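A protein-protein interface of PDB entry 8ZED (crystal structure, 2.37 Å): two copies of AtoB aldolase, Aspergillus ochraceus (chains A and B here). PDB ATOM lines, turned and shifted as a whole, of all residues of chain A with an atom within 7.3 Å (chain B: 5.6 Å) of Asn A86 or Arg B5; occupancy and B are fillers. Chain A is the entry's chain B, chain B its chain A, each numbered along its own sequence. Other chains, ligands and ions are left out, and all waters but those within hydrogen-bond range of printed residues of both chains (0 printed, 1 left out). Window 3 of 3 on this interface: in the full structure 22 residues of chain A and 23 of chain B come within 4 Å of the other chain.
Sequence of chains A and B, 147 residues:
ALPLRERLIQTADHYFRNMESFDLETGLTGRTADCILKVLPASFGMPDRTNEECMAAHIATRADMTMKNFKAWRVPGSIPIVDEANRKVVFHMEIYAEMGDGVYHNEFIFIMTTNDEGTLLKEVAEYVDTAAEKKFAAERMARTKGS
NH2 of Arg B5 lies within salt-bridge range of OD2 of Asp A83, at 2.7 Å.
NH2 of Arg B5 lies close to ND2 of Asn A86 (3.0 Å).
ND2 of Asn A86 lies within hydrogen-bond range of O of Pro B80 (3.4 Å).
The backbone NH (N) of Val B82 is in hydrogen-bond range of the side-chain carboxylate (OD2) of Asp A83.
OD1 of Asp A83 lies close to N of Ala A85, at 3.4 Å.
The side-chain carboxylate (OD2) of Asp A83 lies within hydrogen-bond range of the side-chain amide nitrogen (ND2) of Asn A86, 2.9 Å away.
The backbone NH (N) of Asp A83 sits at hydrogen-bond distance from the backbone carbonyl oxygen (O) of Lys A88 (2.8 Å).
NZ of Lys A88 is in hydrogen-bond range of OG1 of Thr A113, 2.8 Å away.
Among the printed residues, pairs that only touch across the chains: Val A82 with Val B82, Asp A83 with Pro B80, Asp A83 with Ile B81, Asn A86 with Ile B79, Lys A88 with Ile B79 and Lys A88 with Ile B81.
Asn A86 touches just these residues of chain B: Arg B5, Ile B79 and Pro B80.
Of chain A, only Asp A83 and Asn A86 come within 4 Å of Arg B5.
Of the printed residues of chain A, Ile B81 touches Asp A83 (3.7 Å) and Lys A88 (3.7 Å).
Printed residues of chain B within 4 Å of Asp A83: Arg B5 (2.7 Å), Pro B80 (3.8 Å), Ile B81 (3.7 Å) and Val B82 (2.9 Å).
The nearest residue of chain B that does not touch Asn A86 is Ile B81 (4.7 Å).
The nearest residue of chain A that does not touch Arg B5 is Ala A85 (4.4 Å).
Printed residues of chain A that touch a printed residue of chain B: Val A82, Asp A83, Asn A86 and Lys A88.
Along chain A the printed residues that touch a printed residue of chain B span positions 82 to 88.
Among the printed residues, 10 pairs touch across the chains.
Val A82 touches its own counterpart, Val B82.
Positions printed for both chains: 8, 82 and 84.
Of the 10 pairs that touch across the chains among the printed residues, 1 has its exchanged pair printed and touching as well.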
ATOM      1  N   LEU A   8      30.913 -21.170 -18.713  1.00  0.00           N
ATOM      2  CA  LEU A   8      31.102 -21.338 -17.275  1.00  0.00           C
ATOM      3  C   LEU A   8      31.734 -22.688 -16.956  1.00  0.00           C
ATOM      4  O   LEU A   8      32.561 -22.792 -16.042  1.00  0.00           O
ATOM      5  CB  LEU A   8      29.770 -21.186 -16.541  1.00  0.00           C
ATOM      6  CG  LEU A   8      29.114 -19.802 -16.536  1.00  0.00           C
ATOM      7  CD1 LEU A   8      27.857 -19.808 -15.677  1.00  0.00           C
ATOM      8  CD2 LEU A   8      30.090 -18.739 -16.064  1.00  0.00           C
ATOM      9  N   VAL A  82      24.937 -26.060 -13.321  1.00  0.00           N
ATOM     10  CA  VAL A  82      25.266 -24.703 -13.745  1.00  0.00           C
ATOM     11  C   VAL A  82      24.103 -23.778 -13.413  1.00  0.00           C
ATOM     12  O   VAL A  82      22.963 -24.034 -13.817  1.00  0.00           O
ATOM     13  CB  VAL A  82      25.592 -24.641 -15.248  1.00  0.00           C
ATOM     14  CG1 VAL A  82      25.908 -23.212 -15.663  1.00  0.00           C
ATOM     15  CG2 VAL A  82      26.749 -25.569 -15.580  1.00  0.00           C
ATOM     16  N   ASP A  83      24.399 -22.703 -12.686  1.00  0.00           N
ATOM     17  CA  ASP A  83      23.451 -21.625 -12.414  1.00  0.00           C
ATOM     18  C   ASP A  83      24.004 -20.379 -13.100  1.00  0.00           C
ATOM     19  O   ASP A  83      24.883 -19.702 -12.560  1.00  0.00           O
ATOM     20  CB  ASP A  83      23.273 -21.416 -10.911  1.00  0.00           C
ATOM     21  CG  ASP A  83      22.104 -20.501 -10.575  1.00  0.00           C
ATOM     22  OD1 ASP A  83      21.672 -19.721 -11.450  1.00  0.00           O
ATOM     23  OD2 ASP A  83      21.617 -20.562  -9.426  1.00  0.00           O
ATOM     24  N   GLU A  84      23.488 -20.082 -14.297  1.00  0.00           N
ATOM     25  CA  GLU A  84      24.024 -18.972 -15.079  1.00  0.00           C
ATOM     26  C   GLU A  84      23.786 -17.635 -14.387  1.00  0.00           C
ATOM     27  O   GLU A  84      24.651 -16.750 -14.418  1.00  0.00           O
ATOM     28  CB  GLU A  84      23.409 -18.962 -16.478  1.00  0.00           C
ATOM     29  CG  GLU A  84      23.702 -20.203 -17.308  1.00  0.00           C
ATOM     30  CD  GLU A  84      23.264 -20.053 -18.752  1.00  0.00           C
ATOM     31  OE1 GLU A  84      23.260 -18.911 -19.258  1.00  0.00           O
ATOM     32  OE2 GLU A  84      22.920 -21.075 -19.382  1.00  0.00           O
ATOM     33  N   ALA A  85      22.619 -17.467 -13.759  1.00  0.00           N
ATOM     34  CA  ALA A  85      22.307 -16.199 -13.108  1.00  0.00           C
ATOM     35  C   ALA A  85      23.245 -15.918 -11.941  1.00  0.00           C
ATOM     36  O   ALA A  85      23.597 -14.758 -11.695  1.00  0.00           O
ATOM     37  CB  ALA A  85      20.853 -16.196 -12.634  1.00  0.00           C
ATOM     38  N   ASN A  86      23.659 -16.953 -11.218  1.00  0.00           N
ATOM     39  CA  ASN A  86      24.577 -16.799 -10.097  1.00  0.00           C
ATOM     40  C   ASN A  86      26.035 -16.995 -10.488  1.00  0.00           C
ATOM     41  O   ASN A  86      26.913 -16.829  -9.632  1.00  0.00           O
ATOM     42  CB  ASN A  86      24.214 -17.776  -8.975  1.00  0.00           C
ATOM     43  CG  ASN A  86      22.983 -17.346  -8.202  1.00  0.00           C
ATOM     44  OD1 ASN A  86      22.682 -16.157  -8.103  1.00  0.00           O
ATOM     45  ND2 ASN A  86      22.269 -18.315  -7.640  1.00  0.00           N
ATOM     46  N   ARG A  87      26.312 -17.339 -11.748  1.00  0.00           N
ATOM     47  CA  ARG A  87      27.674 -17.593 -12.222  1.00  0.00           C
ATOM     48  C   ARG A  87      28.350 -18.682 -11.389  1.00  0.00           C
ATOM     49  O   ARG A  87      29.508 -18.559 -10.986  1.00  0.00           O
ATOM     50  CB  ARG A  87      28.509 -16.309 -12.222  1.00  0.00           C
ATOM     51  CG  ARG A  87      27.922 -15.164 -13.030  1.00  0.00           C
ATOM     52  CD  ARG A  87      27.870 -15.491 -14.512  1.00  0.00           C
ATOM     53  NE  ARG A  87      27.572 -14.311 -15.314  1.00  0.00           N
ATOM     54  CZ  ARG A  87      26.350 -13.867 -15.572  1.00  0.00           C
ATOM     55  NH1 ARG A  87      25.277 -14.485 -15.106  1.00  0.00           N
ATOM     56  NH2 ARG A  87      26.198 -12.774 -16.315  1.00  0.00           N
ATOM     57  N   LYS A  88      27.611 -19.759 -11.127  1.00  0.00           N
ATOM     58  CA  LYS A  88      28.092 -20.837 -10.275  1.00  0.00           C
ATOM     59  C   LYS A  88      28.025 -22.168 -11.008  1.00  0.00           C
ATOM     60  O   LYS A  88      27.061 -22.445 -11.729  1.00  0.00           O
ATOM     61  CB  LYS A  88      27.288 -20.918  -8.971  1.00  0.00           C
ATOM     62  CG  LYS A  88      27.481 -19.718  -8.059  1.00  0.00           C
ATOM     63  CD  LYS A  88      26.926 -19.977  -6.671  1.00  0.00           C
ATOM     64  CE  LYS A  88      27.085 -18.757  -5.779  1.00  0.00           C
ATOM     65  NZ  LYS A  88      28.507 -18.330  -5.667  1.00  0.00           N
ATOM     66  N   VAL A  89      29.058 -22.987 -10.816  1.00  0.00           N
ATOM     67  CA  VAL A  89      29.137 -24.328 -11.384  1.00  0.00           C
ATOM     68  C   VAL A  89      29.502 -25.295 -10.266  1.00  0.00           C
ATOM     69  O   VAL A  89      30.428 -25.032  -9.491  1.00  0.00           O
ATOM     70  CB  VAL A  89      30.167 -24.412 -12.527  1.00  0.00           C
ATOM     71  CG1 VAL A  89      30.222 -25.824 -13.088  1.00  0.00           C
ATOM     72  CG2 VAL A  89      29.832 -23.415 -13.625  1.00  0.00           C
ATOM     73  N   MET A 112      32.259 -23.579  -7.912  1.00  0.00           N
ATOM     74  CA  MET A 112      33.015 -22.502  -8.529  1.00  0.00           C
ATOM     75  C   MET A 112      32.125 -21.287  -8.754  1.00  0.00           C
ATOM     76  O   MET A 112      30.930 -21.413  -9.033  1.00  0.00           O
ATOM     77  CB  MET A 112      33.624 -22.945  -9.864  1.00  0.00           C
ATOM     78  CG  MET A 112      34.913 -23.741  -9.741  1.00  0.00           C
ATOM     79  SD  MET A 112      34.685 -25.391  -9.059  1.00  0.00           S
ATOM     80  CE  MET A 112      36.356 -26.023  -9.181  1.00  0.00           C
ATOM     81  N   THR A 113      32.726 -20.106  -8.628  1.00  0.00           N
ATOM     82  CA  THR A 113      32.060 -18.844  -8.915  1.00  0.00           C
ATOM     83  C   THR A 113      32.926 -18.052  -9.882  1.00  0.00           C
ATOM     84  O   THR A 113      34.137 -17.924  -9.673  1.00  0.00           O
ATOM     85  CB  THR A 113      31.813 -18.031  -7.638  1.00  0.00           C
ATOM     86  OG1 THR A 113      31.045 -18.810  -6.713  1.00  0.00           O
ATOM     87  CG2 THR A 113      31.056 -16.749  -7.959  1.00  0.00           C
ATOM     88  N   THR A 114      32.309 -17.526 -10.933  1.00  0.00           N
ATOM     89  CA  THR A 114      33.013 -16.787 -11.967  1.00  0.00           C
ATOM     90  C   THR A 114      32.655 -15.309 -11.903  1.00  0.00           C
ATOM     91  O   THR A 114      31.761 -14.885 -11.165  1.00  0.00           O
ATOM     92  CB  THR A 114      32.683 -17.343 -13.356  1.00  0.00           C
ATOM     93  OG1 THR A 114      31.350 -16.961 -13.713  1.00  0.00           O
ATOM     94  CG2 THR A 114      32.790 -18.861 -13.363  1.00  0.00           C
ATOM     95  N   ASN A 115      33.371 -14.520 -12.701  1.00  0.00           N
ATOM     96  CA  ASN A 115      33.060 -13.108 -12.843  1.00  0.00           C
ATOM     97  C   ASN A 115      31.806 -12.936 -13.702  1.00  0.00           C
ATOM     98  O   ASN A 115      31.223 -13.899 -14.207  1.00  0.00           O
ATOM     99  CB  ASN A 115      34.247 -12.361 -13.444  1.00  0.00           C
ATOM    100  CG  ASN A 115      34.808 -13.047 -14.678  1.00  0.00           C
ATOM    101  OD1 ASN A 115      34.239 -14.017 -15.180  1.00  0.00           O
ATOM    102  ND2 ASN A 115      35.932 -12.542 -15.174  1.00  0.00           N
ATOM    103  N   LYS A 122      36.361 -16.488  -9.629  1.00  0.00           N
ATOM    104  CA  LYS A 122      36.334 -15.569  -8.499  1.00  0.00           C
ATOM    105  C   LYS A 122      36.387 -16.278  -7.154  1.00  0.00           C
ATOM    106  O   LYS A 122      36.919 -15.717  -6.190  1.00  0.00           O
ATOM    107  CB  LYS A 122      35.072 -14.700  -8.552  1.00  0.00           C
ATOM    108  CG  LYS A 122      35.034 -13.583  -7.520  1.00  0.00           C
ATOM    109  CD  LYS A 122      33.606 -13.172  -7.200  1.00  0.00           C
ATOM    110  CE  LYS A 122      32.842 -12.777  -8.453  1.00  0.00           C
ATOM    111  NZ  LYS A 122      31.424 -12.440  -8.148  1.00  0.00           N
ATOM    112  N   PRO B   3       7.312 -19.391 -10.855  1.00  0.00           N
ATOM    113  CA  PRO B   3       8.456 -19.557 -11.756  1.00  0.00           C
ATOM    114  C   PRO B   3       9.224 -20.825 -11.414  1.00  0.00           C
ATOM    115  O   PRO B   3       9.295 -21.239 -10.255  1.00  0.00           O
ATOM    116  CB  PRO B   3       9.297 -18.302 -11.499  1.00  0.00           C
ATOM    117  CG  PRO B   3       8.322 -17.299 -10.980  1.00  0.00           C
ATOM    118  CD  PRO B   3       7.323 -18.082 -10.180  1.00  0.00           C
ATOM    119  N   LEU B   4       9.799 -21.445 -12.448  1.00  0.00           N
ATOM    120  CA  LEU B   4      10.449 -22.740 -12.261  1.00  0.00           C
ATOM    121  C   LEU B   4      11.612 -22.645 -11.279  1.00  0.00           C
ATOM    122  O   LEU B   4      11.854 -23.578 -10.505  1.00  0.00           O
ATOM    123  CB  LEU B   4      10.923 -23.290 -13.606  1.00  0.00           C
ATOM    124  CG  LEU B   4      11.579 -24.673 -13.556  1.00  0.00           C
ATOM    125  CD1 LEU B   4      10.650 -25.682 -12.895  1.00  0.00           C
ATOM    126  CD2 LEU B   4      11.974 -25.134 -14.950  1.00  0.00           C
ATOM    127  N   ARG B   5      12.338 -21.526 -11.292  1.00  0.00           N
ATOM    128  CA  ARG B   5      13.450 -21.359 -10.360  1.00  0.00           C
ATOM    129  C   ARG B   5      12.959 -21.350  -8.918  1.00  0.00           C
ATOM    130  O   ARG B   5      13.536 -22.011  -8.047  1.00  0.00           O
ATOM    131  CB  ARG B   5      14.217 -20.075 -10.671  1.00  0.00           C
ATOM    132  CG  ARG B   5      15.421 -19.857  -9.769  1.00  0.00           C
ATOM    133  CD  ARG B   5      16.169 -18.582 -10.115  1.00  0.00           C
ATOM    134  NE  ARG B   5      17.383 -18.450  -9.320  1.00  0.00           N
ATOM    135  CZ  ARG B   5      18.562 -18.949  -9.668  1.00  0.00           C
ATOM    136  NH1 ARG B   5      18.727 -19.603 -10.805  1.00  0.00           N
ATOM    137  NH2 ARG B   5      19.600 -18.789  -8.854  1.00  0.00           N
ATOM    138  N   GLU B   6      11.886 -20.603  -8.646  1.00  0.00           N
ATOM    139  CA  GLU B   6      11.355 -20.552  -7.289  1.00  0.00           C
ATOM    140  C   GLU B   6      10.681 -21.866  -6.911  1.00  0.00           C
ATOM    141  O   GLU B   6      10.827 -22.338  -5.779  1.00  0.00           O
ATOM    142  CB  GLU B   6      10.376 -19.385  -7.149  1.00  0.00           C
ATOM    143  CG  GLU B   6       9.892 -19.152  -5.726  1.00  0.00           C
ATOM    144  CD  GLU B   6       8.904 -18.006  -5.624  1.00  0.00           C
ATOM    145  OE1 GLU B   6       8.382 -17.574  -6.672  1.00  0.00           O
ATOM    146  OE2 GLU B   6       8.651 -17.536  -4.494  1.00  0.00           O
ATOM    147  N   ARG B   7       9.949 -22.474  -7.850  1.00  0.00           N
ATOM    148  CA  ARG B   7       9.270 -23.732  -7.556  1.00  0.00           C
ATOM    149  C   ARG B   7      10.266 -24.838  -7.228  1.00  0.00           C
ATOM    150  O   ARG B   7       9.997 -25.695  -6.378  1.00  0.00           O
ATOM    151  CB  ARG B   7       8.378 -24.138  -8.731  1.00  0.00           C
ATOM    152  CG  ARG B   7       7.566 -25.399  -8.474  1.00  0.00           C
ATOM    153  CD  ARG B   7       6.355 -25.506  -9.392  1.00  0.00           C
ATOM    154  NE  ARG B   7       6.707 -25.869 -10.760  1.00  0.00           N
ATOM    155  CZ  ARG B   7       6.704 -25.027 -11.784  1.00  0.00           C
ATOM    156  NH1 ARG B   7       6.380 -23.753 -11.633  1.00  0.00           N
ATOM    157  NH2 ARG B   7       7.029 -25.476 -12.994  1.00  0.00           N
ATOM    158  N   LEU B   8      11.428 -24.833  -7.888  1.00  0.00           N
ATOM    159  CA  LEU B   8      12.464 -25.804  -7.552  1.00  0.00           C
ATOM    160  C   LEU B   8      13.003 -25.577  -6.145  1.00  0.00           C
ATOM    161  O   LEU B   8      13.369 -26.537  -5.457  1.00  0.00           O
ATOM    162  CB  LEU B   8      13.601 -25.740  -8.574  1.00  0.00           C
ATOM    163  CG  LEU B   8      13.336 -26.328  -9.964  1.00  0.00           C
ATOM    164  CD1 LEU B   8      14.465 -25.979 -10.922  1.00  0.00           C
ATOM    165  CD2 LEU B   8      13.151 -27.832  -9.886  1.00  0.00           C
ATOM    166  N   ILE B   9      13.051 -24.321  -5.699  1.00  0.00           N
ATOM    167  CA  ILE B   9      13.552 -24.026  -4.360  1.00  0.00           C
ATOM    168  C   ILE B   9      12.541 -24.453  -3.302  1.00  0.00           C
ATOM    169  O   ILE B   9      12.911 -25.014  -2.264  1.00  0.00           O
ATOM    170  CB  ILE B   9      13.905 -22.532  -4.242  1.00  0.00           C
ATOM    171  CG1 ILE B   9      15.041 -22.181  -5.205  1.00  0.00           C
ATOM    172  CG2 ILE B   9      14.283 -22.176  -2.812  1.00  0.00           C
ATOM    173  CD1 ILE B   9      15.426 -20.718  -5.191  1.00  0.00           C
ATOM    174  N   GLN B  10      11.252 -24.201  -3.549  1.00  0.00           N
ATOM    175  CA  GLN B  10      10.220 -24.614  -2.602  1.00  0.00           C
ATOM    176  C   GLN B  10      10.191 -26.130  -2.446  1.00  0.00           C
ATOM    177  O   GLN B  10      10.075 -26.645  -1.327  1.00  0.00           O
ATOM    178  CB  GLN B  10       8.852 -24.104  -3.058  1.00  0.00           C
ATOM    179  CG  GLN B  10       8.814 -22.631  -3.443  1.00  0.00           C
ATOM    180  CD  GLN B  10       8.802 -21.703  -2.246  1.00  0.00           C
ATOM    181  OE1 GLN B  10       8.322 -22.061  -1.171  1.00  0.00           O
ATOM    182  NE2 GLN B  10       9.329 -20.497  -2.429  1.00  0.00           N
ATOM    183  N   ILE B  79      23.577 -18.759  -1.111  1.00  0.00           N
ATOM    184  CA  ILE B  79      22.378 -18.635  -1.936  1.00  0.00           C
ATOM    185  C   ILE B  79      22.065 -19.985  -2.571  1.00  0.00           C
ATOM    186  O   ILE B  79      22.983 -20.788  -2.800  1.00  0.00           O
ATOM    187  CB  ILE B  79      22.548 -17.544  -3.004  1.00  0.00           C
ATOM    188  CG1 ILE B  79      23.759 -17.849  -3.889  1.00  0.00           C
ATOM    189  CG2 ILE B  79      22.691 -16.177  -2.353  1.00  0.00           C
ATOM    190  CD1 ILE B  79      24.034 -16.791  -4.933  1.00  0.00           C
ATOM    191  N   PRO B  80      20.799 -20.286  -2.857  1.00  0.00           N
ATOM    192  CA  PRO B  80      20.475 -21.555  -3.524  1.00  0.00           C
ATOM    193  C   PRO B  80      21.012 -21.580  -4.948  1.00  0.00           C
ATOM    194  O   PRO B  80      20.759 -20.669  -5.740  1.00  0.00           O
ATOM    195  CB  PRO B  80      18.941 -21.589  -3.500  1.00  0.00           C
ATOM    196  CG  PRO B  80      18.552 -20.647  -2.401  1.00  0.00           C
ATOM    197  CD  PRO B  80      19.589 -19.567  -2.424  1.00  0.00           C
ATOM    198  N   ILE B  81      21.756 -22.635  -5.268  1.00  0.00           N
ATOM    199  CA  ILE B  81      22.268 -22.857  -6.616  1.00  0.00           C
ATOM    200  C   ILE B  81      21.242 -23.703  -7.360  1.00  0.00           C
ATOM    201  O   ILE B  81      21.014 -24.864  -7.010  1.00  0.00           O
ATOM    202  CB  ILE B  81      23.642 -23.537  -6.594  1.00  0.00           C
ATOM    203  CG1 ILE B  81      24.637 -22.705  -5.778  1.00  0.00           C
ATOM    204  CG2 ILE B  81      24.151 -23.756  -8.009  1.00  0.00           C
ATOM    205  CD1 ILE B  81      25.982 -23.374  -5.590  1.00  0.00           C
ATOM    206  N   VAL B  82      20.624 -23.128  -8.391  1.00  0.00           N
ATOM    207  CA  VAL B  82      19.524 -23.760  -9.109  1.00  0.00           C
ATOM    208  C   VAL B  82      19.913 -23.932 -10.571  1.00  0.00           C
ATOM    209  O   VAL B  82      20.294 -22.962 -11.235  1.00  0.00           O
ATOM    210  CB  VAL B  82      18.225 -22.941  -8.989  1.00  0.00           C
ATOM    211  CG1 VAL B  82      17.091 -23.630  -9.732  1.00  0.00           C
ATOM    212  CG2 VAL B  82      17.862 -22.725  -7.527  1.00  0.00           C
ATOM    213  N   GLU B  84      17.907 -25.035 -13.670  1.00  0.00           N
ATOM    214  CA  GLU B  84      16.546 -25.340 -14.106  1.00  0.00           C
ATOM    215  C   GLU B  84      16.526 -26.456 -15.142  1.00  0.00           C
ATOM    216  O   GLU B  84      15.608 -27.285 -15.152  1.00  0.00           O
ATOM    217  CB  GLU B  84      15.877 -24.085 -14.667  1.00  0.00           C
ATOM    218  CG  GLU B  84      15.680 -22.967 -13.659  1.00  0.00           C
ATOM    219  CD  GLU B  84      14.875 -21.814 -14.228  1.00  0.00           C
ATOM    220  OE1 GLU B  84      14.114 -22.039 -15.193  1.00  0.00           O
ATOM    221  OE2 GLU B  84      15.006 -20.683 -13.716  1.00  0.00           O
